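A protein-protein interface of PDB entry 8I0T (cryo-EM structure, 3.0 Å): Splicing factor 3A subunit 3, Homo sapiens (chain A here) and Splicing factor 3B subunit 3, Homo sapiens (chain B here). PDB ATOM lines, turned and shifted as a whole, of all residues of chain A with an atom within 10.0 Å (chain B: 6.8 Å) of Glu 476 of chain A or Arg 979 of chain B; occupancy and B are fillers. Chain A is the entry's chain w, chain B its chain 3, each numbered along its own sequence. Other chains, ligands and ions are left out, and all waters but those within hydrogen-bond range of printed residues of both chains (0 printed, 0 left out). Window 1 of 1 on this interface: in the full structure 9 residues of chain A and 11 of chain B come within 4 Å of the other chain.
Among the printed residues, merely in contact across the chains: Trp 471 of chain A with Lys 980 of chain B, Trp 471 of chain A with Cys 981 of chain B, Trp 471 of chain A with Glu 982 of chain B, Glu 476 of chain A with Arg 979 of chain B, Glu 476 of chain A with Glu 982 of chain B, Glu 477 of chain A with Arg 979 of chain B, Glu 478 of chain A with Leu 977 of chain B, Glu 478 of chain A with Leu 978 of chain B, Glu 478 of chain A with Lys 980 of chain B and Val 486 of chain A with Leu 978 of chain B.
The guanidinium group (NH2) of Arg 979 of chain B is in salt-bridge range of the side-chain carboxylate (OE1) of Glu 478 of chain A (3.0 Å). The side-chain amino group (NZ) of Lys 984 of chain B lies close to the backbone carbonyl oxygen (O) of Arg 470 of chain A (3.5 Å). NZ of Lys 984 of chain B lies close to O of Glu 469 of chain A (2.3 Å). The backbone NH of Trp 471 of chain A sits close to the side-chain amino group of Lys 984 of chain B, 3.0 Å away.
Glu 476 of chain A touches just these residues of chain B: Arg 979 and Glu 982. Of chain A, only Glu 478 (3.2 Å) and Val 486 (3.7 Å) come within 4 Å of Leu 978 of chain B. Of chain A, only Trp 471 (3.0 Å) and Glu 478 (3.9 Å) come within 4 Å of Lys 980 of chain B. Of chain A, only Trp 471 (3.7 Å) and Glu 476 (3.2 Å) come within 4 Å of Glu 982 of chain B. Of the printed residues of chain B, Glu 469 of chain A touches Lys 984 (2.3 Å). Printed residues of chain A within 4 Å of Cys 981 of chain B: Trp 471 (3.6 Å). Of the printed residues of chain B, Glu 478 of chain A touches Leu 977 (3.7 Å), Leu 978 (3.2 Å), Arg 979 (3.0 Å) and Lys 980 (3.9 Å). Printed residues of chain B within 4 Å of Glu 477 of chain A: Arg 979 (3.3 Å). Gln 472 of chain A touches none of the printed residues of chain B. Pro 473 of chain A touches none of the printed residues of chain B. The nearest residue of chain A that does not touch Arg 979 of chain B is Trp 471 of chain A (4.8 Å).
Of the 12 printed residues of chain B, 7 touch a printed residue of chain A. Printed residues of chain B that touch a printed residue of chain A: Leu 977, Leu 978, Arg 979, Lys 980, Cys 981, Glu 982 and Lys 984. Hydrophobic or aromatic side chains of chain B within 4 Å of the printed part of chain A: Leu 978. Hydrophobic or aromatic side chains of chain A within 4 Å of the printed part of chain B: Trp 471 and Val 486. Among the printed residues, 14 pairs touch across the chains.
N of Lys 980 of chain B is in hydrogen-bond range of O of Val 969 of chain B (2.8 Å). N of Val 969 of chain B is in hydrogen-bond range of O of Cys 981 of chain B, at 2.9 Å. The backbone NH of Asp 971 of chain B sits at hydrogen-bond distance from the backbone carbonyl oxygen of Leu 978 of chain B (2.9 Å). The side-chain amide oxygen (OE1) of Gln 472 of chain A lies close to the backbone carbonyl oxygen (O) of Arg 470 of chain A. The side-chain amide oxygen (OE1) of Gln 472 of chain A lies close to the side-chain carboxylate (OE1) of Glu 476 of chain A (3.4 Å). O of Glu 477 of chain A sits at hydrogen-bond distance from N of Lys 489 of chain A, 2.7 Å away.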
ATOM      1  N   GLN A 465      -7.519  23.603  33.660  1.00  0.00           N
ATOM      2  CA  GLN A 465      -7.427  22.461  32.754  1.00  0.00           C
ATOM      3  C   GLN A 465      -8.716  21.645  32.766  1.00  0.00           C
ATOM      4  O   GLN A 465      -9.157  21.137  31.727  1.00  0.00           O
ATOM      5  CB  GLN A 465      -6.215  21.597  33.121  1.00  0.00           C
ATOM      6  CG  GLN A 465      -4.871  22.226  32.739  1.00  0.00           C
ATOM      7  CD  GLN A 465      -3.664  21.403  33.182  1.00  0.00           C
ATOM      8  OE1 GLN A 465      -3.745  20.612  34.122  1.00  0.00           O
ATOM      9  NE2 GLN A 465      -2.538  21.590  32.500  1.00  0.00           N
ATOM     10  N   LYS A 466      -9.331  21.496  33.940  1.00  0.00           N
ATOM     11  CA  LYS A 466     -10.594  20.768  34.009  1.00  0.00           C
ATOM     12  C   LYS A 466     -11.682  21.482  33.226  1.00  0.00           C
ATOM     13  O   LYS A 466     -12.446  20.841  32.493  1.00  0.00           O
ATOM     14  CB  LYS A 466     -11.020  20.577  35.463  1.00  0.00           C
ATOM     15  CG  LYS A 466     -12.478  20.168  35.640  1.00  0.00           C
ATOM     16  CD  LYS A 466     -12.652  19.229  36.820  1.00  0.00           C
ATOM     17  CE  LYS A 466     -11.680  18.064  36.720  1.00  0.00           C
ATOM     18  NZ  LYS A 466     -11.785  17.129  37.868  1.00  0.00           N
ATOM     19  N   ALA A 467     -11.749  22.810  33.355  1.00  0.00           N
ATOM     20  CA  ALA A 467     -12.713  23.588  32.583  1.00  0.00           C
ATOM     21  C   ALA A 467     -12.397  23.533  31.098  1.00  0.00           C
ATOM     22  O   ALA A 467     -13.304  23.539  30.262  1.00  0.00           O
ATOM     23  CB  ALA A 467     -12.729  25.034  33.069  1.00  0.00           C
ATOM     24  N   SER A 468     -11.109  23.502  30.751  1.00  0.00           N
ATOM     25  CA  SER A 468     -10.716  23.342  29.358  1.00  0.00           C
ATOM     26  C   SER A 468     -11.276  22.047  28.784  1.00  0.00           C
ATOM     27  O   SER A 468     -12.108  22.060  27.870  1.00  0.00           O
ATOM     28  CB  SER A 468      -9.185  23.353  29.245  1.00  0.00           C
ATOM     29  OG  SER A 468      -8.578  24.133  30.260  1.00  0.00           O
ATOM     30  N   GLU A 469     -10.835  20.915  29.332  1.00  0.00           N
ATOM     31  CA  GLU A 469     -11.168  19.614  28.762  1.00  0.00           C
ATOM     32  C   GLU A 469     -12.623  19.224  28.974  1.00  0.00           C
ATOM     33  O   GLU A 469     -13.085  18.263  28.351  1.00  0.00           O
ATOM     34  CB  GLU A 469     -10.232  18.550  29.319  1.00  0.00           C
ATOM     35  CG  GLU A 469      -8.800  18.803  28.898  1.00  0.00           C
ATOM     36  CD  GLU A 469      -8.716  19.584  27.587  1.00  0.00           C
ATOM     37  OE1 GLU A 469      -8.856  18.966  26.514  1.00  0.00           O
ATOM     38  OE2 GLU A 469      -8.518  20.814  27.617  1.00  0.00           O
ATOM     39  N   ARG A 470     -13.349  19.924  29.837  1.00  0.00           N
ATOM     40  CA  ARG A 470     -14.792  19.806  29.773  1.00  0.00           C
ATOM     41  C   ARG A 470     -15.276  20.267  28.404  1.00  0.00           C
ATOM     42  O   ARG A 470     -14.783  21.249  27.845  1.00  0.00           O
ATOM     43  CB  ARG A 470     -15.465  20.646  30.860  1.00  0.00           C
ATOM     44  CG  ARG A 470     -15.494  20.045  32.246  1.00  0.00           C
ATOM     45  CD  ARG A 470     -16.450  20.843  33.104  1.00  0.00           C
ATOM     46  NE  ARG A 470     -17.266  19.997  33.966  1.00  0.00           N
ATOM     47  CZ  ARG A 470     -18.043  20.463  34.938  1.00  0.00           C
ATOM     48  NH1 ARG A 470     -18.106  21.766  35.166  1.00  0.00           N
ATOM     49  NH2 ARG A 470     -18.757  19.631  35.686  1.00  0.00           N
ATOM     50  N   TRP A 471     -16.226  19.526  27.846  1.00  0.00           N
ATOM     51  CA  TRP A 471     -16.948  19.967  26.659  1.00  0.00           C
ATOM     52  C   TRP A 471     -18.200  20.665  27.160  1.00  0.00           C
ATOM     53  O   TRP A 471     -19.066  20.038  27.777  1.00  0.00           O
ATOM     54  CB  TRP A 471     -17.256  18.806  25.711  1.00  0.00           C
ATOM     55  CG  TRP A 471     -18.687  18.639  25.327  1.00  0.00           C
ATOM     56  CD1 TRP A 471     -19.601  17.844  25.936  1.00  0.00           C
ATOM     57  CD2 TRP A 471     -19.367  19.272  24.240  1.00  0.00           C
ATOM     58  NE1 TRP A 471     -20.811  17.942  25.306  1.00  0.00           N
ATOM     59  CE2 TRP A 471     -20.692  18.813  24.257  1.00  0.00           C
ATOM     60  CE3 TRP A 471     -18.985  20.181  23.258  1.00  0.00           C
ATOM     61  CZ2 TRP A 471     -21.639  19.236  23.334  1.00  0.00           C
ATOM     62  CZ3 TRP A 471     -19.928  20.597  22.342  1.00  0.00           C
ATOM     63  CH2 TRP A 471     -21.238  20.129  22.388  1.00  0.00           C
ATOM     64  N   GLN A 472     -18.259  21.975  26.962  1.00  0.00           N
ATOM     65  CA  GLN A 472     -19.399  22.757  27.404  1.00  0.00           C
ATOM     66  C   GLN A 472     -20.248  23.068  26.187  1.00  0.00           C
ATOM     67  O   GLN A 472     -19.801  23.808  25.293  1.00  0.00           O
ATOM     68  CB  GLN A 472     -18.960  24.046  28.097  1.00  0.00           C
ATOM     69  CG  GLN A 472     -17.819  23.862  29.073  1.00  0.00           C
ATOM     70  CD  GLN A 472     -16.477  24.109  28.419  1.00  0.00           C
ATOM     71  OE1 GLN A 472     -16.116  23.436  27.458  1.00  0.00           O
ATOM     72  NE2 GLN A 472     -15.740  25.088  28.923  1.00  0.00           N
ATOM     73  N   PRO A 473     -21.463  22.538  26.111  1.00  0.00           N
ATOM     74  CA  PRO A 473     -22.288  22.785  24.922  1.00  0.00           C
ATOM     75  C   PRO A 473     -22.667  24.242  24.761  1.00  0.00           C
ATOM     76  O   PRO A 473     -22.929  24.687  23.640  1.00  0.00           O
ATOM     77  CB  PRO A 473     -23.513  21.890  25.158  1.00  0.00           C
ATOM     78  CG  PRO A 473     -23.143  20.996  26.329  1.00  0.00           C
ATOM     79  CD  PRO A 473     -22.172  21.767  27.138  1.00  0.00           C
ATOM     80  N   ASP A 474     -22.670  25.008  25.853  1.00  0.00           N
ATOM     81  CA  ASP A 474     -23.061  26.408  25.772  1.00  0.00           C
ATOM     82  C   ASP A 474     -22.165  27.198  24.826  1.00  0.00           C
ATOM     83  O   ASP A 474     -22.658  27.826  23.882  1.00  0.00           O
ATOM     84  CB  ASP A 474     -23.049  27.030  27.166  1.00  0.00           C
ATOM     85  CG  ASP A 474     -24.438  27.330  27.675  1.00  0.00           C
ATOM     86  OD1 ASP A 474     -24.585  27.582  28.888  1.00  0.00           O
ATOM     87  OD2 ASP A 474     -25.383  27.319  26.860  1.00  0.00           O
ATOM     88  N   THR A 475     -20.853  27.175  25.048  1.00  0.00           N
ATOM     89  CA  THR A 475     -19.951  27.891  24.159  1.00  0.00           C
ATOM     90  C   THR A 475     -19.532  27.070  22.946  1.00  0.00           C
ATOM     91  O   THR A 475     -19.286  27.644  21.885  1.00  0.00           O
ATOM     92  CB  THR A 475     -18.690  28.342  24.904  1.00  0.00           C
ATOM     93  OG1 THR A 475     -17.678  27.338  24.768  1.00  0.00           O
ATOM     94  CG2 THR A 475     -18.989  28.570  26.380  1.00  0.00           C
ATOM     95  N   GLU A 476     -19.458  25.738  23.059  1.00  0.00           N
ATOM     96  CA  GLU A 476     -19.079  24.969  21.878  1.00  0.00           C
ATOM     97  C   GLU A 476     -20.267  24.731  20.945  1.00  0.00           C
ATOM     98  O   GLU A 476     -20.268  25.209  19.806  1.00  0.00           O
ATOM     99  CB  GLU A 476     -18.443  23.637  22.299  1.00  0.00           C
ATOM    100  CG  GLU A 476     -17.470  23.730  23.472  1.00  0.00           C
ATOM    101  CD  GLU A 476     -16.346  22.701  23.409  1.00  0.00           C
ATOM    102  OE1 GLU A 476     -15.394  22.805  24.213  1.00  0.00           O
ATOM    103  OE2 GLU A 476     -16.411  21.790  22.558  1.00  0.00           O
ATOM    104  N   GLU A 477     -21.292  24.019  21.421  1.00  0.00           N
ATOM    105  CA  GLU A 477     -22.473  23.693  20.632  1.00  0.00           C
ATOM    106  C   GLU A 477     -23.086  24.968  20.077  1.00  0.00           C
ATOM    107  O   GLU A 477     -23.545  25.823  20.837  1.00  0.00           O
ATOM    108  CB  GLU A 477     -23.484  22.927  21.490  1.00  0.00           C
ATOM    109  CG  GLU A 477     -24.871  22.764  20.878  1.00  0.00           C
ATOM    110  CD  GLU A 477     -25.797  21.929  21.751  1.00  0.00           C
ATOM    111  OE1 GLU A 477     -26.349  20.928  21.258  1.00  0.00           O
ATOM    112  OE2 GLU A 477     -25.963  22.278  22.932  1.00  0.00           O
ATOM    113  N   GLU A 478     -23.097  25.098  18.759  1.00  0.00           N
ATOM    114  CA  GLU A 478     -23.317  26.376  18.101  1.00  0.00           C
ATOM    115  C   GLU A 478     -24.414  26.261  17.053  1.00  0.00           C
ATOM    116  O   GLU A 478     -24.536  25.232  16.383  1.00  0.00           O
ATOM    117  CB  GLU A 478     -22.011  26.859  17.477  1.00  0.00           C
ATOM    118  CG  GLU A 478     -21.379  25.847  16.543  1.00  0.00           C
ATOM    119  CD  GLU A 478     -20.244  26.440  15.751  1.00  0.00           C
ATOM    120  OE1 GLU A 478     -19.240  26.841  16.371  1.00  0.00           O
ATOM    121  OE2 GLU A 478     -20.358  26.517  14.513  1.00  0.00           O
ATOM    122  N   TYR A 479     -25.199  27.326  16.908  1.00  0.00           N
ATOM    123  CA  TYR A 479     -26.420  27.310  16.111  1.00  0.00           C
ATOM    124  C   TYR A 479     -26.422  28.476  15.139  1.00  0.00           C
ATOM    125  O   TYR A 479     -26.222  29.624  15.543  1.00  0.00           O
ATOM    126  CB  TYR A 479     -27.670  27.423  16.988  1.00  0.00           C
ATOM    127  CG  TYR A 479     -28.036  26.205  17.804  1.00  0.00           C
ATOM    128  CD1 TYR A 479     -29.297  25.644  17.709  1.00  0.00           C
ATOM    129  CD2 TYR A 479     -27.140  25.644  18.696  1.00  0.00           C
ATOM    130  CE1 TYR A 479     -29.651  24.552  18.467  1.00  0.00           C
ATOM    131  CE2 TYR A 479     -27.482  24.555  19.452  1.00  0.00           C
ATOM    132  CZ  TYR A 479     -28.741  24.011  19.338  1.00  0.00           C
ATOM    133  OH  TYR A 479     -29.090  22.919  20.093  1.00  0.00           O
ATOM    134  N   GLU A 480     -26.674  28.180  13.869  1.00  0.00           N
ATOM    135  CA  GLU A 480     -27.028  29.205  12.902  1.00  0.00           C
ATOM    136  C   GLU A 480     -28.483  29.614  13.098  1.00  0.00           C
ATOM    137  O   GLU A 480     -29.360  28.767  13.286  1.00  0.00           O
ATOM    138  CB  GLU A 480     -26.826  28.710  11.470  1.00  0.00           C
ATOM    139  CG  GLU A 480     -27.689  27.504  11.117  1.00  0.00           C
ATOM    140  CD  GLU A 480     -28.197  27.531   9.695  1.00  0.00           C
ATOM    141  OE1 GLU A 480     -27.444  27.939   8.787  1.00  0.00           O
ATOM    142  OE2 GLU A 480     -29.361  27.135   9.486  1.00  0.00           O
ATOM    143  N   VAL A 486     -24.455  32.601  12.329  1.00  0.00           N
ATOM    144  CA  VAL A 486     -24.364  31.567  13.351  1.00  0.00           C
ATOM    145  C   VAL A 486     -24.139  32.195  14.716  1.00  0.00           C
ATOM    146  O   VAL A 486     -23.487  33.240  14.841  1.00  0.00           O
ATOM    147  CB  VAL A 486     -23.242  30.568  13.017  1.00  0.00           C
ATOM    148  CG1 VAL A 486     -21.893  31.251  13.090  1.00  0.00           C
ATOM    149  CG2 VAL A 486     -23.298  29.365  13.944  1.00  0.00           C
ATOM    150  N   VAL A 487     -24.704  31.558  15.742  1.00  0.00           N
ATOM    151  CA  VAL A 487     -24.454  31.869  17.139  1.00  0.00           C
ATOM    152  C   VAL A 487     -24.269  30.557  17.880  1.00  0.00           C
ATOM    153  O   VAL A 487     -24.207  29.480  17.283  1.00  0.00           O
ATOM    154  CB  VAL A 487     -25.582  32.692  17.778  1.00  0.00           C
ATOM    155  CG1 VAL A 487     -25.376  34.157  17.497  1.00  0.00           C
ATOM    156  CG2 VAL A 487     -26.906  32.247  17.214  1.00  0.00           C
ATOM    157  N   ASN A 488     -24.148  30.664  19.197  1.00  0.00           N
ATOM    158  CA  ASN A 488     -24.017  29.478  20.019  1.00  0.00           C
ATOM    159  C   ASN A 488     -25.387  28.944  20.421  1.00  0.00           C
ATOM    160  O   ASN A 488     -26.427  29.550  20.152  1.00  0.00           O
ATOM    161  CB  ASN A 488     -23.194  29.774  21.268  1.00  0.00           C
ATOM    162  CG  ASN A 488     -23.518  31.120  21.866  1.00  0.00           C
ATOM    163  OD1 ASN A 488     -24.514  31.276  22.571  1.00  0.00           O
ATOM    164  ND2 ASN A 488     -22.668  32.103  21.601  1.00  0.00           N
ATOM    165  N   LYS A 489     -25.367  27.773  21.061  1.00  0.00           N
ATOM    166  CA  LYS A 489     -26.571  27.236  21.679  1.00  0.00           C
ATOM    167  C   LYS A 489     -27.234  28.251  22.587  1.00  0.00           C
ATOM    168  O   LYS A 489     -28.449  28.489  22.484  1.00  0.00           O
ATOM    169  CB  LYS A 489     -26.231  25.986  22.485  1.00  0.00           C
ATOM    170  CG  LYS A 489     -27.416  25.367  23.212  1.00  0.00           C
ATOM    171  CD  LYS A 489     -27.590  25.898  24.641  1.00  0.00           C
ATOM    172  CE  LYS A 489     -29.068  26.115  24.954  1.00  0.00           C
ATOM    173  NZ  LYS A 489     -29.310  26.689  26.299  1.00  0.00           N
ATOM    174  N   LYS A 490     -26.461  28.825  23.508  1.00  0.00           N
ATOM    175  CA  LYS A 490     -27.013  29.716  24.513  1.00  0.00           C
ATOM    176  C   LYS A 490     -27.742  30.858  23.825  1.00  0.00           C
ATOM    177  O   LYS A 490     -28.964  30.950  23.935  1.00  0.00           O
ATOM    178  CB  LYS A 490     -25.914  30.231  25.449  1.00  0.00           C
ATOM    179  CG  LYS A 490     -26.466  30.824  26.733  1.00  0.00           C
ATOM    180  CD  LYS A 490     -25.560  30.600  27.931  1.00  0.00           C
ATOM    181  CE  LYS A 490     -24.238  31.328  27.806  1.00  0.00           C
ATOM    182  NZ  LYS A 490     -23.684  31.666  29.152  1.00  0.00           N
ATOM    183  N   THR A 491     -27.013  31.676  23.059  1.00  0.00           N
ATOM    184  CA  THR A 491     -27.618  32.849  22.437  1.00  0.00           C
ATOM    185  C   THR A 491     -28.754  32.467  21.501  1.00  0.00           C
ATOM    186  O   THR A 491     -29.747  33.204  21.394  1.00  0.00           O
ATOM    187  CB  THR A 491     -26.572  33.646  21.672  1.00  0.00           C
ATOM    188  OG1 THR A 491     -25.394  33.795  22.475  1.00  0.00           O
ATOM    189  CG2 THR A 491     -27.126  35.021  21.323  1.00  0.00           C
ATOM    190  N   ARG B 968     -14.429  15.725  16.967  1.00  0.00           N
ATOM    191  CA  ARG B 968     -15.578  16.602  17.089  1.00  0.00           C
ATOM    192  C   ARG B 968     -16.664  16.216  16.101  1.00  0.00           C
ATOM    193  O   ARG B 968     -16.396  15.839  14.955  1.00  0.00           O
ATOM    194  CB  ARG B 968     -15.186  18.058  16.898  1.00  0.00           C
ATOM    195  CG  ARG B 968     -13.990  18.456  17.685  1.00  0.00           C
ATOM    196  CD  ARG B 968     -13.078  19.267  16.820  1.00  0.00           C
ATOM    197  NE  ARG B 968     -13.160  20.693  17.095  1.00  0.00           N
ATOM    198  CZ  ARG B 968     -12.621  21.618  16.315  1.00  0.00           C
ATOM    199  NH1 ARG B 968     -11.969  21.253  15.229  1.00  0.00           N
ATOM    200  NH2 ARG B 968     -12.719  22.899  16.626  1.00  0.00           N
ATOM    201  N   VAL B 969     -17.898  16.338  16.572  1.00  0.00           N
ATOM    202  CA  VAL B 969     -19.085  15.903  15.858  1.00  0.00           C
ATOM    203  C   VAL B 969     -19.728  17.141  15.268  1.00  0.00           C
ATOM    204  O   VAL B 969     -19.967  18.122  15.984  1.00  0.00           O
ATOM    205  CB  VAL B 969     -20.054  15.162  16.786  1.00  0.00           C
ATOM    206  CG1 VAL B 969     -21.480  15.330  16.323  1.00  0.00           C
ATOM    207  CG2 VAL B 969     -19.683  13.718  16.849  1.00  0.00           C
ATOM    208  N   TYR B 970     -20.002  17.088  13.966  1.00  0.00           N
ATOM    209  CA  TYR B 970     -20.434  18.229  13.184  1.00  0.00           C
ATOM    210  C   TYR B 970     -21.775  17.961  12.523  1.00  0.00           C
ATOM    211  O   TYR B 970     -22.034  16.868  11.994  1.00  0.00           O
ATOM    212  CB  TYR B 970     -19.419  18.571  12.099  1.00  0.00           C
ATOM    213  CG  TYR B 970     -18.170  19.215  12.621  1.00  0.00           C
ATOM    214  CD1 TYR B 970     -17.791  20.475  12.196  1.00  0.00           C
ATOM    215  CD2 TYR B 970     -17.359  18.560  13.534  1.00  0.00           C
ATOM    216  CE1 TYR B 970     -16.647  21.064  12.675  1.00  0.00           C
ATOM    217  CE2 TYR B 970     -16.220  19.138  14.007  1.00  0.00           C
ATOM    218  CZ  TYR B 970     -15.866  20.388  13.582  1.00  0.00           C
ATOM    219  OH  TYR B 970     -14.719  20.962  14.071  1.00  0.00           O
ATOM    220  N   ASP B 971     -22.601  19.004  12.540  1.00  0.00           N
ATOM    221  CA  ASP B 971     -23.837  19.097  11.792  1.00  0.00           C
ATOM    222  C   ASP B 971     -23.793  20.391  10.992  1.00  0.00           C
ATOM    223  O   ASP B 971     -22.879  21.209  11.139  1.00  0.00           O
ATOM    224  CB  ASP B 971     -25.062  19.055  12.704  1.00  0.00           C
ATOM    225  CG  ASP B 971     -26.210  18.280  12.099  1.00  0.00           C
ATOM    226  OD1 ASP B 971     -26.137  17.948  10.903  1.00  0.00           O
ATOM    227  OD2 ASP B 971     -27.184  17.989  12.820  1.00  0.00           O
ATOM    228  N   LEU B 977     -19.847  25.137   8.983  1.00  0.00           N
ATOM    229  CA  LEU B 977     -20.192  23.860   9.600  1.00  0.00           C
ATOM    230  C   LEU B 977     -20.145  23.968  11.119  1.00  0.00           C
ATOM    231  O   LEU B 977     -19.147  24.401  11.698  1.00  0.00           O
ATOM    232  CB  LEU B 977     -19.220  22.778   9.143  1.00  0.00           C
ATOM    233  CG  LEU B 977     -19.728  21.632   8.282  1.00  0.00           C
ATOM    234  CD1 LEU B 977     -18.664  20.544   8.285  1.00  0.00           C
ATOM    235  CD2 LEU B 977     -21.073  21.104   8.747  1.00  0.00           C
ATOM    236  N   LEU B 978     -21.224  23.542  11.774  1.00  0.00           N
ATOM    237  CA  LEU B 978     -21.432  23.825  13.186  1.00  0.00           C
ATOM    238  C   LEU B 978     -21.234  22.572  14.024  1.00  0.00           C
ATOM    239  O   LEU B 978     -21.716  21.492  13.677  1.00  0.00           O
ATOM    240  CB  LEU B 978     -22.828  24.403  13.412  1.00  0.00           C
ATOM    241  CG  LEU B 978     -23.474  24.813  12.089  1.00  0.00           C
ATOM    242  CD1 LEU B 978     -24.869  24.275  12.000  1.00  0.00           C
ATOM    243  CD2 LEU B 978     -23.474  26.320  11.926  1.00  0.00           C
ATOM    244  N   ARG B 979     -20.556  22.739  15.150  1.00  0.00           N
ATOM    245  CA  ARG B 979     -20.047  21.625  15.940  1.00  0.00           C
ATOM    246  C   ARG B 979     -21.010  21.326  17.074  1.00  0.00           C
ATOM    247  O   ARG B 979     -21.206  22.139  17.976  1.00  0.00           O
ATOM    248  CB  ARG B 979     -18.661  21.957  16.465  1.00  0.00           C
ATOM    249  CG  ARG B 979     -18.312  21.328  17.793  1.00  0.00           C
ATOM    250  CD  ARG B 979     -17.021  21.933  18.320  1.00  0.00           C
ATOM    251  NE  ARG B 979     -17.172  23.368  18.545  1.00  0.00           N
ATOM    252  CZ  ARG B 979     -16.799  24.313  17.691  1.00  0.00           C
ATOM    253  NH1 ARG B 979     -16.236  23.996  16.533  1.00  0.00           N
ATOM    254  NH2 ARG B 979     -16.998  25.585  17.998  1.00  0.00           N
ATOM    255  N   LYS B 980     -21.622  20.153  17.017  1.00  0.00           N
ATOM    256  CA  LYS B 980     -22.560  19.712  18.034  1.00  0.00           C
ATOM    257  C   LYS B 980     -21.924  18.855  19.118  1.00  0.00           C
ATOM    258  O   LYS B 980     -22.565  18.622  20.148  1.00  0.00           O
ATOM    259  CB  LYS B 980     -23.706  18.933  17.386  1.00  0.00           C
ATOM    260  CG  LYS B 980     -24.513  19.768  16.416  1.00  0.00           C
ATOM    261  CD  LYS B 980     -24.728  21.164  16.960  1.00  0.00           C
ATOM    262  CE  LYS B 980     -26.069  21.701  16.534  1.00  0.00           C
ATOM    263  NZ  LYS B 980     -26.145  21.814  15.057  1.00  0.00           N
ATOM    264  N   CYS B 981     -20.705  18.358  18.922  1.00  0.00           N
ATOM    265  CA  CYS B 981     -20.051  17.633  20.007  1.00  0.00           C
ATOM    266  C   CYS B 981     -18.546  17.789  19.890  1.00  0.00           C
ATOM    267  O   CYS B 981     -18.013  18.105  18.826  1.00  0.00           O
ATOM    268  CB  CYS B 981     -20.415  16.149  20.010  1.00  0.00           C
ATOM    269  SG  CYS B 981     -21.605  15.656  21.237  1.00  0.00           S
ATOM    270  N   GLU B 982     -17.864  17.510  20.996  1.00  0.00           N
ATOM    271  CA  GLU B 982     -16.412  17.496  21.026  1.00  0.00           C
ATOM    272  C   GLU B 982     -15.968  16.464  22.045  1.00  0.00           C
ATOM    273  O   GLU B 982     -16.622  16.291  23.073  1.00  0.00           O
ATOM    274  CB  GLU B 982     -15.844  18.878  21.386  1.00  0.00           C
ATOM    275  CG  GLU B 982     -14.322  18.917  21.548  1.00  0.00           C
ATOM    276  CD  GLU B 982     -13.652  20.081  20.820  1.00  0.00           C
ATOM    277  OE1 GLU B 982     -14.226  20.587  19.839  1.00  0.00           O
ATOM    278  OE2 GLU B 982     -12.546  20.490  21.229  1.00  0.00           O
ATOM    279  N   ASN B 983     -14.886  15.762  21.742  1.00  0.00           N
ATOM    280  CA  ASN B 983     -14.156  15.004  22.742  1.00  0.00           C
ATOM    281  C   ASN B 983     -12.683  15.314  22.580  1.00  0.00           C
ATOM    282  O   ASN B 983     -12.190  15.489  21.461  1.00  0.00           O
ATOM    283  CB  ASN B 983     -14.379  13.508  22.635  1.00  0.00           C
ATOM    284  CG  ASN B 983     -13.763  12.757  23.797  1.00  0.00           C
ATOM    285  OD1 ASN B 983     -12.564  12.852  24.050  1.00  0.00           O
ATOM    286  ND2 ASN B 983     -14.590  12.031  24.535  1.00  0.00           N
ATOM    287  N   LYS B 984     -11.981  15.367  23.705  1.00  0.00           N
ATOM    288  CA  LYS B 984     -10.654  15.953  23.744  1.00  0.00           C
ATOM    289  C   LYS B 984      -9.615  15.042  24.369  1.00  0.00           C
ATOM    290  O   LYS B 984      -8.561  15.526  24.784  1.00  0.00           O
ATOM    291  CB  LYS B 984     -10.716  17.277  24.503  1.00  0.00           C
ATOM    292  CG  LYS B 984     -11.717  18.256  23.917  1.00  0.00           C
ATOM    293  CD  LYS B 984     -12.130  19.302  24.922  1.00  0.00           C
ATOM    294  CE  LYS B 984     -13.624  19.274  25.161  1.00  0.00           C
ATOM    295  NZ  LYS B 984     -14.018  18.301  26.204  1.00  0.00           N
